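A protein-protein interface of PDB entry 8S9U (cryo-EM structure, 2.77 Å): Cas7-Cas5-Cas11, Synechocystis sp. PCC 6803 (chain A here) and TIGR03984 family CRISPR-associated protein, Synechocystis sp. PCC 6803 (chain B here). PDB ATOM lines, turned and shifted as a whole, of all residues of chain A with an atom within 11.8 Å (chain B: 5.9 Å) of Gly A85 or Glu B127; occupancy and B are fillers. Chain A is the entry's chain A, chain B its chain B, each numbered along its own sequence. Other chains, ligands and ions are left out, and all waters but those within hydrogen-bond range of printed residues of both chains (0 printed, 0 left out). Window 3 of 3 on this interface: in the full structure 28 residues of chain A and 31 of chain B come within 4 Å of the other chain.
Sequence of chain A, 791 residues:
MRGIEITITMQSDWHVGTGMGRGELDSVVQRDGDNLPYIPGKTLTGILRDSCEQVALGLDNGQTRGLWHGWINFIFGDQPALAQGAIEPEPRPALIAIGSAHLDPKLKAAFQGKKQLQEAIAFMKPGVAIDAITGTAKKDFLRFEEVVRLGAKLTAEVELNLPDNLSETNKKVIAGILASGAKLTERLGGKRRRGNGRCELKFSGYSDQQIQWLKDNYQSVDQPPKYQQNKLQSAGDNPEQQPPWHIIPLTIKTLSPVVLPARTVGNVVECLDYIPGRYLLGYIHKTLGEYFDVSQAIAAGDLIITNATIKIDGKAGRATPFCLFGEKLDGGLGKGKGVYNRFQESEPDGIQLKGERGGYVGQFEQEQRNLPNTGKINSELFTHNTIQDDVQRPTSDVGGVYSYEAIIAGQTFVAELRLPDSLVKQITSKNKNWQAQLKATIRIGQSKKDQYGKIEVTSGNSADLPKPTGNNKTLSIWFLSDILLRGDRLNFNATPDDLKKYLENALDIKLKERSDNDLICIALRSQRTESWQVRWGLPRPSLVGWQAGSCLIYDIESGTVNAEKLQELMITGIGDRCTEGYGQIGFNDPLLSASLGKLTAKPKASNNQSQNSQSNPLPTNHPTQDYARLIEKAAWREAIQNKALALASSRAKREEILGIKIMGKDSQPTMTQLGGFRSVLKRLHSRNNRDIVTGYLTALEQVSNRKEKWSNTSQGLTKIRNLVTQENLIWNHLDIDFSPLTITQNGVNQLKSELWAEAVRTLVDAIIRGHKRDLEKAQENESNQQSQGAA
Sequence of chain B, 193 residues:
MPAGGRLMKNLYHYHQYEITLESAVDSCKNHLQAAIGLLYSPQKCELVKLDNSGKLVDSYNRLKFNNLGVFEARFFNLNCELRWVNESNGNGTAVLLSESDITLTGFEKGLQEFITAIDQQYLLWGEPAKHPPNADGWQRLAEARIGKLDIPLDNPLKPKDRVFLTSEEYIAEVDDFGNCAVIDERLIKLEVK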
ATOM      1  N   ARG A  65      -0.715  -1.459  -7.428  1.00  0.00           N
ATOM      2  CA  ARG A  65      -0.265  -1.395  -8.808  1.00  0.00           C
ATOM      3  C   ARG A  65       0.772  -2.484  -9.016  1.00  0.00           C
ATOM      4  O   ARG A  65       1.576  -2.758  -8.125  1.00  0.00           O
ATOM      5  CB  ARG A  65       0.325  -0.027  -9.154  1.00  0.00           C
ATOM      6  CG  ARG A  65      -0.654   1.126  -9.010  1.00  0.00           C
ATOM      7  CD  ARG A  65      -0.064   2.407  -9.563  1.00  0.00           C
ATOM      8  NE  ARG A  65      -0.953   3.551  -9.385  1.00  0.00           N
ATOM      9  CZ  ARG A  65      -0.622   4.802  -9.688  1.00  0.00           C
ATOM     10  NH1 ARG A  65       0.590   5.072 -10.152  1.00  0.00           N
ATOM     11  NH2 ARG A  65      -1.488   5.788  -9.499  1.00  0.00           N
ATOM     12  N   GLN A  79      -7.844   4.604 -16.387  1.00  0.00           N
ATOM     13  CA  GLN A  79      -8.748   5.609 -15.848  1.00  0.00           C
ATOM     14  C   GLN A  79      -8.052   6.953 -15.701  1.00  0.00           C
ATOM     15  O   GLN A  79      -7.651   7.323 -14.595  1.00  0.00           O
ATOM     16  CB  GLN A  79      -9.289   5.147 -14.506  1.00  0.00           C
ATOM     17  CG  GLN A  79      -9.904   3.795 -14.580  1.00  0.00           C
ATOM     18  CD  GLN A  79     -10.543   3.397 -13.302  1.00  0.00           C
ATOM     19  OE1 GLN A  79     -11.736   3.585 -13.106  1.00  0.00           O
ATOM     20  NE2 GLN A  79      -9.754   2.840 -12.406  1.00  0.00           N
ATOM     21  N   PRO A  80      -7.876   7.701 -16.788  1.00  0.00           N
ATOM     22  CA  PRO A  80      -7.084   8.934 -16.720  1.00  0.00           C
ATOM     23  C   PRO A  80      -7.643  10.005 -15.804  1.00  0.00           C
ATOM     24  O   PRO A  80      -6.900  10.915 -15.430  1.00  0.00           O
ATOM     25  CB  PRO A  80      -7.075   9.406 -18.175  1.00  0.00           C
ATOM     26  CG  PRO A  80      -8.246   8.768 -18.769  1.00  0.00           C
ATOM     27  CD  PRO A  80      -8.338   7.447 -18.156  1.00  0.00           C
ATOM     28  N   ALA A  81      -8.917   9.939 -15.428  1.00  0.00           N
ATOM     29  CA  ALA A  81      -9.462  10.942 -14.523  1.00  0.00           C
ATOM     30  C   ALA A  81      -8.968  10.774 -13.097  1.00  0.00           C
ATOM     31  O   ALA A  81      -9.056  11.716 -12.308  1.00  0.00           O
ATOM     32  CB  ALA A  81     -10.987  10.896 -14.548  1.00  0.00           C
ATOM     33  N   LEU A  82      -8.455   9.601 -12.750  1.00  0.00           N
ATOM     34  CA  LEU A  82      -7.882   9.400 -11.429  1.00  0.00           C
ATOM     35  C   LEU A  82      -6.434   9.856 -11.385  1.00  0.00           C
ATOM     36  O   LEU A  82      -6.037  10.602 -10.486  1.00  0.00           O
ATOM     37  CB  LEU A  82      -7.985   7.931 -11.032  1.00  0.00           C
ATOM     38  CG  LEU A  82      -9.398   7.370 -11.014  1.00  0.00           C
ATOM     39  CD1 LEU A  82      -9.378   5.974 -10.445  1.00  0.00           C
ATOM     40  CD2 LEU A  82     -10.318   8.271 -10.232  1.00  0.00           C
ATOM     41  N   ALA A  83      -5.637   9.422 -12.356  1.00  0.00           N
ATOM     42  CA  ALA A  83      -4.212   9.707 -12.350  1.00  0.00           C
ATOM     43  C   ALA A  83      -3.950  11.198 -12.463  1.00  0.00           C
ATOM     44  O   ALA A  83      -4.692  11.939 -13.111  1.00  0.00           O
ATOM     45  CB  ALA A  83      -3.523   8.980 -13.499  1.00  0.00           C
ATOM     46  N   GLN A  84      -2.873  11.636 -11.820  1.00  0.00           N
ATOM     47  CA  GLN A  84      -2.548  13.047 -11.720  1.00  0.00           C
ATOM     48  C   GLN A  84      -1.040  13.210 -11.810  1.00  0.00           C
ATOM     49  O   GLN A  84      -0.277  12.292 -11.507  1.00  0.00           O
ATOM     50  CB  GLN A  84      -3.085  13.655 -10.424  1.00  0.00           C
ATOM     51  CG  GLN A  84      -2.426  13.120  -9.176  1.00  0.00           C
ATOM     52  CD  GLN A  84      -3.078  13.641  -7.914  1.00  0.00           C
ATOM     53  OE1 GLN A  84      -4.048  14.395  -7.970  1.00  0.00           O
ATOM     54  NE2 GLN A  84      -2.543  13.247  -6.766  1.00  0.00           N
ATOM     55  N   GLY A  85      -0.623  14.392 -12.219  1.00  0.00           N
ATOM     56  CA  GLY A  85       0.734  14.606 -12.655  1.00  0.00           C
ATOM     57  C   GLY A  85       0.970  14.197 -14.098  1.00  0.00           C
ATOM     58  O   GLY A  85       0.053  13.910 -14.870  1.00  0.00           O
ATOM     59  N   ALA A  86       2.253  14.189 -14.461  1.00  0.00           N
ATOM     60  CA  ALA A  86       2.699  13.990 -15.840  1.00  0.00           C
ATOM     61  C   ALA A  86       2.671  12.517 -16.248  1.00  0.00           C
ATOM     62  O   ALA A  86       3.703  11.874 -16.446  1.00  0.00           O
ATOM     63  CB  ALA A  86       4.089  14.573 -16.019  1.00  0.00           C
ATOM     64  N   ILE A  87       1.464  11.972 -16.372  1.00  0.00           N
ATOM     65  CA  ILE A  87       1.317  10.640 -16.956  1.00  0.00           C
ATOM     66  C   ILE A  87       1.573  10.755 -18.455  1.00  0.00           C
ATOM     67  O   ILE A  87       0.788  11.365 -19.181  1.00  0.00           O
ATOM     68  CB  ILE A  87      -0.058  10.033 -16.667  1.00  0.00           C
ATOM     69  CG1 ILE A  87      -0.147   9.552 -15.221  1.00  0.00           C
ATOM     70  CG2 ILE A  87      -0.318   8.870 -17.589  1.00  0.00           C
ATOM     71  CD1 ILE A  87      -0.226  10.640 -14.196  1.00  0.00           C
ATOM     72  N   GLU A  88       2.672  10.172 -18.918  1.00  0.00           N
ATOM     73  CA  GLU A  88       3.099  10.286 -20.308  1.00  0.00           C
ATOM     74  C   GLU A  88       2.350   9.428 -21.325  1.00  0.00           C
ATOM     75  O   GLU A  88       2.073   9.914 -22.426  1.00  0.00           O
ATOM     76  CB  GLU A  88       4.593   9.989 -20.408  1.00  0.00           C
ATOM     77  CG  GLU A  88       5.467  11.102 -19.886  1.00  0.00           C
ATOM     78  CD  GLU A  88       6.933  10.839 -20.128  1.00  0.00           C
ATOM     79  OE1 GLU A  88       7.345  10.822 -21.305  1.00  0.00           O
ATOM     80  OE2 GLU A  88       7.679  10.661 -19.143  1.00  0.00           O
ATOM     81  N   PRO A  89       2.029   8.164 -21.047  1.00  0.00           N
ATOM     82  CA  PRO A  89       1.346   7.361 -22.068  1.00  0.00           C
ATOM     83  C   PRO A  89      -0.084   7.822 -22.300  1.00  0.00           C
ATOM     84  O   PRO A  89      -0.793   8.211 -21.369  1.00  0.00           O
ATOM     85  CB  PRO A  89       1.396   5.942 -21.496  1.00  0.00           C
ATOM     86  CG  PRO A  89       1.521   6.130 -20.055  1.00  0.00           C
ATOM     87  CD  PRO A  89       2.355   7.349 -19.867  1.00  0.00           C
ATOM     88  N   GLU A  90      -0.500   7.772 -23.558  1.00  0.00           N
ATOM     89  CA  GLU A  90      -1.895   7.994 -23.900  1.00  0.00           C
ATOM     90  C   GLU A  90      -2.782   6.954 -23.224  1.00  0.00           C
ATOM     91  O   GLU A  90      -2.384   5.795 -23.082  1.00  0.00           O
ATOM     92  CB  GLU A  90      -2.082   7.951 -25.415  1.00  0.00           C
ATOM     93  CG  GLU A  90      -1.279   9.005 -26.153  1.00  0.00           C
ATOM     94  CD  GLU A  90       0.089   8.511 -26.593  1.00  0.00           C
ATOM     95  OE1 GLU A  90       0.554   8.930 -27.674  1.00  0.00           O
ATOM     96  OE2 GLU A  90       0.699   7.708 -25.856  1.00  0.00           O
ATOM     97  N   PRO A  91      -3.977   7.336 -22.779  1.00  0.00           N
ATOM     98  CA  PRO A  91      -4.855   6.382 -22.091  1.00  0.00           C
ATOM     99  C   PRO A  91      -5.351   5.277 -23.012  1.00  0.00           C
ATOM    100  O   PRO A  91      -5.881   5.538 -24.091  1.00  0.00           O
ATOM    101  CB  PRO A  91      -6.001   7.265 -21.589  1.00  0.00           C
ATOM    102  CG  PRO A  91      -5.999   8.427 -22.473  1.00  0.00           C
ATOM    103  CD  PRO A  91      -4.591   8.665 -22.886  1.00  0.00           C
ATOM    104  N   LEU A 538      -6.086  14.940 -29.398  1.00  0.00           N
ATOM    105  CA  LEU A 538      -6.179  16.345 -29.050  1.00  0.00           C
ATOM    106  C   LEU A 538      -7.514  16.838 -29.567  1.00  0.00           C
ATOM    107  O   LEU A 538      -8.074  16.252 -30.496  1.00  0.00           O
ATOM    108  CB  LEU A 538      -5.043  17.158 -29.675  1.00  0.00           C
ATOM    109  CG  LEU A 538      -3.644  16.929 -29.135  1.00  0.00           C
ATOM    110  CD1 LEU A 538      -2.673  17.727 -29.945  1.00  0.00           C
ATOM    111  CD2 LEU A 538      -3.593  17.343 -27.699  1.00  0.00           C
ATOM    112  N   TRP B 125      -1.772  21.814 -22.629  1.00  0.00           N
ATOM    113  CA  TRP B 125      -2.131  20.583 -21.947  1.00  0.00           C
ATOM    114  C   TRP B 125      -0.940  20.016 -21.197  1.00  0.00           C
ATOM    115  O   TRP B 125       0.100  19.748 -21.803  1.00  0.00           O
ATOM    116  CB  TRP B 125      -2.560  19.536 -22.964  1.00  0.00           C
ATOM    117  CG  TRP B 125      -3.864  19.639 -23.606  1.00  0.00           C
ATOM    118  CD1 TRP B 125      -4.109  19.926 -24.902  1.00  0.00           C
ATOM    119  CD2 TRP B 125      -5.121  19.334 -23.016  1.00  0.00           C
ATOM    120  NE1 TRP B 125      -5.452  19.876 -25.151  1.00  0.00           N
ATOM    121  CE2 TRP B 125      -6.096  19.511 -24.001  1.00  0.00           C
ATOM    122  CE3 TRP B 125      -5.519  18.956 -21.739  1.00  0.00           C
ATOM    123  CZ2 TRP B 125      -7.440  19.322 -23.751  1.00  0.00           C
ATOM    124  CZ3 TRP B 125      -6.840  18.775 -21.498  1.00  0.00           C
ATOM    125  CH2 TRP B 125      -7.789  18.953 -22.492  1.00  0.00           C
ATOM    126  N   GLY B 126      -1.075  19.814 -19.900  1.00  0.00           N
ATOM    127  CA  GLY B 126      -0.007  19.073 -19.270  1.00  0.00           C
ATOM    128  C   GLY B 126       0.824  19.914 -18.318  1.00  0.00           C
ATOM    129  O   GLY B 126       0.855  21.146 -18.379  1.00  0.00           O
ATOM    130  N   GLU B 127       1.464  19.235 -17.440  1.00  0.00           N
ATOM    131  CA  GLU B 127       2.480  19.629 -16.495  1.00  0.00           C
ATOM    132  C   GLU B 127       3.835  19.164 -17.008  1.00  0.00           C
ATOM    133  O   GLU B 127       3.915  18.172 -17.733  1.00  0.00           O
ATOM    134  CB  GLU B 127       2.222  19.005 -15.123  1.00  0.00           C
ATOM    135  CG  GLU B 127       0.870  19.322 -14.538  1.00  0.00           C
ATOM    136  CD  GLU B 127       0.728  18.831 -13.114  1.00  0.00           C
ATOM    137  OE1 GLU B 127       1.603  19.153 -12.286  1.00  0.00           O
ATOM    138  OE2 GLU B 127      -0.257  18.127 -12.819  1.00  0.00           O
ATOM    139  N   PRO B 128       4.916  19.852 -16.664  1.00  0.00           N
ATOM    140  CA  PRO B 128       6.241  19.425 -17.128  1.00  0.00           C
ATOM    141  C   PRO B 128       6.564  17.983 -16.789  1.00  0.00           C
ATOM    142  O   PRO B 128       6.486  17.581 -15.627  1.00  0.00           O
ATOM    143  CB  PRO B 128       7.180  20.392 -16.407  1.00  0.00           C
ATOM    144  CG  PRO B 128       6.358  21.604 -16.214  1.00  0.00           C
ATOM    145  CD  PRO B 128       4.980  21.119 -15.926  1.00  0.00           C
ATOM    146  N   ALA B 129       6.908  17.190 -17.795  1.00  0.00           N
ATOM    147  CA  ALA B 129       7.201  15.785 -17.577  1.00  0.00           C
ATOM    148  C   ALA B 129       8.591  15.615 -16.977  1.00  0.00           C
ATOM    149  O   ALA B 129       8.849  14.673 -16.229  1.00  0.00           O
ATOM    150  CB  ALA B 129       7.086  15.018 -18.867  1.00  0.00           C
ATOM    151  N   ARG B 140       8.809  18.460 -22.642  1.00  0.00           N
ATOM    152  CA  ARG B 140       7.608  17.649 -22.639  1.00  0.00           C
ATOM    153  C   ARG B 140       6.662  18.089 -21.538  1.00  0.00           C
ATOM    154  O   ARG B 140       7.052  18.166 -20.371  1.00  0.00           O
ATOM    155  CB  ARG B 140       7.976  16.179 -22.478  1.00  0.00           C
ATOM    156  CG  ARG B 140       6.817  15.245 -22.511  1.00  0.00           C
ATOM    157  CD  ARG B 140       7.321  13.837 -22.568  1.00  0.00           C
ATOM    158  NE  ARG B 140       8.008  13.603 -23.830  1.00  0.00           N
ATOM    159  CZ  ARG B 140       8.753  12.540 -24.088  1.00  0.00           C
ATOM    160  NH1 ARG B 140       8.808  11.542 -23.223  1.00  0.00           N
ATOM    161  NH2 ARG B 140       9.348  12.422 -25.264  1.00  0.00           N
ATOM    162  N   LEU B 141       5.423  18.367 -21.916  1.00  0.00           N
ATOM    163  CA  LEU B 141       4.309  18.387 -20.987  1.00  0.00           C
ATOM    164  C   LEU B 141       3.640  17.025 -21.034  1.00  0.00           C
ATOM    165  O   LEU B 141       3.715  16.321 -22.040  1.00  0.00           O
ATOM    166  CB  LEU B 141       3.317  19.486 -21.350  1.00  0.00           C
ATOM    167  CG  LEU B 141       3.932  20.866 -21.559  1.00  0.00           C
ATOM    168  CD1 LEU B 141       2.889  21.853 -22.014  1.00  0.00           C
ATOM    169  CD2 LEU B 141       4.579  21.342 -20.294  1.00  0.00           C
ATOM    170  N   ALA B 142       2.981  16.646 -19.945  1.00  0.00           N
ATOM    171  CA  ALA B 142       2.123  15.479 -20.031  1.00  0.00           C
ATOM    172  C   ALA B 142       0.928  15.618 -19.111  1.00  0.00           C
ATOM    173  O   ALA B 142       0.981  16.290 -18.082  1.00  0.00           O
ATOM    174  CB  ALA B 142       2.887  14.200 -19.691  1.00  0.00           C
ATOM    175  N   GLU B 143      -0.153  14.959 -19.509  1.00  0.00           N
ATOM    176  CA  GLU B 143      -1.409  14.938 -18.783  1.00  0.00           C
ATOM    177  C   GLU B 143      -2.028  13.571 -18.992  1.00  0.00           C
ATOM    178  O   GLU B 143      -2.008  13.052 -20.107  1.00  0.00           O
ATOM    179  CB  GLU B 143      -2.356  16.024 -19.290  1.00  0.00           C
ATOM    180  CG  GLU B 143      -3.445  16.377 -18.336  1.00  0.00           C
ATOM    181  CD  GLU B 143      -4.130  17.663 -18.708  1.00  0.00           C
ATOM    182  OE1 GLU B 143      -3.424  18.654 -18.976  1.00  0.00           O
ATOM    183  OE2 GLU B 143      -5.376  17.689 -18.711  1.00  0.00           O
ATOM    184  N   ALA B 144      -2.551  12.979 -17.921  1.00  0.00           N
ATOM    185  CA  ALA B 144      -3.166  11.663 -18.050  1.00  0.00           C
ATOM    186  C   ALA B 144      -4.267  11.670 -19.092  1.00  0.00           C
ATOM    187  O   ALA B 144      -4.491  10.666 -19.772  1.00  0.00           O
ATOM    188  CB  ALA B 144      -3.713  11.201 -16.705  1.00  0.00           C
ATOM    189  N   PRO B 159       8.868  21.807 -11.975  1.00  0.00           N
ATOM    190  CA  PRO B 159       7.649  20.996 -11.829  1.00  0.00           C
ATOM    191  C   PRO B 159       6.372  21.795 -11.655  1.00  0.00           C
ATOM    192  O   PRO B 159       5.292  21.292 -11.986  1.00  0.00           O
ATOM    193  CB  PRO B 159       7.950  20.156 -10.583  1.00  0.00           C
ATOM    194  CG  PRO B 159       9.427  20.038 -10.578  1.00  0.00           C
ATOM    195  CD  PRO B 159       9.928  21.368 -11.053  1.00  0.00           C
ATOM    196  N   ASP B 161       5.915  24.863 -13.081  1.00  0.00           N
ATOM    197  CA  ASP B 161       5.688  25.679 -14.262  1.00  0.00           C
ATOM    198  C   ASP B 161       4.514  25.166 -15.081  1.00  0.00           C
ATOM    199  O   ASP B 161       4.212  23.973 -15.104  1.00  0.00           O
ATOM    200  CB  ASP B 161       6.933  25.708 -15.144  1.00  0.00           C
ATOM    201  CG  ASP B 161       8.045  26.545 -14.560  1.00  0.00           C
ATOM    202  OD1 ASP B 161       7.765  27.380 -13.676  1.00  0.00           O
ATOM    203  OD2 ASP B 161       9.205  26.369 -14.991  1.00  0.00           O
ATOM    204  N   ARG B 162       3.844  26.094 -15.745  1.00  0.00           N
ATOM    205  CA  ARG B 162       2.852  25.787 -16.759  1.00  0.00           C
ATOM    206  C   ARG B 162       3.210  26.598 -17.985  1.00  0.00           C
ATOM    207  O   ARG B 162       3.623  27.753 -17.873  1.00  0.00           O
ATOM    208  CB  ARG B 162       1.422  26.111 -16.330  1.00  0.00           C
ATOM    209  CG  ARG B 162       0.972  25.414 -15.088  1.00  0.00           C
ATOM    210  CD  ARG B 162       0.872  23.937 -15.309  1.00  0.00           C
ATOM    211  NE  ARG B 162       0.603  23.246 -14.056  1.00  0.00           N
ATOM    212  CZ  ARG B 162       1.503  22.527 -13.393  1.00  0.00           C
ATOM    213  NH1 ARG B 162       2.748  22.444 -13.839  1.00  0.00           N
ATOM    214  NH2 ARG B 162       1.169  21.927 -12.259  1.00  0.00           N
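O of Ile A87 sits close to O of Glu B143, at 3.4 Å. OE1 of Glu A88 lies within salt-bridge range of NH1 of Arg B140, at 2.5 Å.
The side-chain carboxylate (OE1) of Glu B127 is in salt-bridge range of the guanidinium group (NH2) of Arg B162, at 2.8 Å. The backbone NH (N) of Ala B142 is in hydrogen-bond range of the backbone carbonyl oxygen (O) of Glu B127 (2.8 Å). The backbone NH (N) of Gly B126 is in hydrogen-bond range of the side-chain carboxylate (OE1) of Glu B143 (2.8 Å). The backbone carbonyl oxygen (O) of Arg B140 is in hydrogen-bond range of the backbone NH (N) of Ala B129, 2.8 Å away.
Among the printed residues, merely in contact across the chains: Pro A80 with Ala B144, Ala A83 with Ala B144, Gly A85 with Glu B127, Ala A86 with Glu B127, Ala A86 with Pro B128, Ala A86 with Ala B129, Ala A86 with Ala B142, Ile A87 with Ala B142, Ile A87 with Ala B144, Glu A88 with Ala B142, Pro A91 with Ala B144 and Leu A538 with Trp B125.
Gly A85 touches just one residue of chain B: Glu B127. No residue of chain A comes within 4 Å of Gly B126. Printed residues of chain A within 4 Å of Ala B129: Ala A86 (3.7 Å). No residue of chain A comes within 4 Å of Leu B141. Ala B142 touches three residues of chain A. Of the printed residues of chain A, Glu B143 touches Ile A87 (3.4 Å). Of the printed residues of chain B, Leu A538 touches Trp B125 (3.8 Å). Of the printed residues of chain B, Ala A86 touches Glu B127, Pro B128, Ala B129 and Ala B142. Glu A90 touches none of the printed residues of chain B. The nearest printed residue of chain B that does not touch Gly A85 is Ala B142 (4.1 Å).
Printed residues of chain A that touch a printed residue of chain B: Pro A80, Ala A83, Gly A85, Ala A86, Ile A87, Glu A88, Pro A91 and Leu A538. Of the 13 printed residues of chain B, 8 touch a printed residue of chain A. Among the printed residues, 14 pairs touch across the chains. Among the printed residues, Asp or Glu carboxylates within 4 Å of a Lys or Arg side-chain nitrogen of the other chain: Glu A88 with Arg B140 (2.5 Å).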
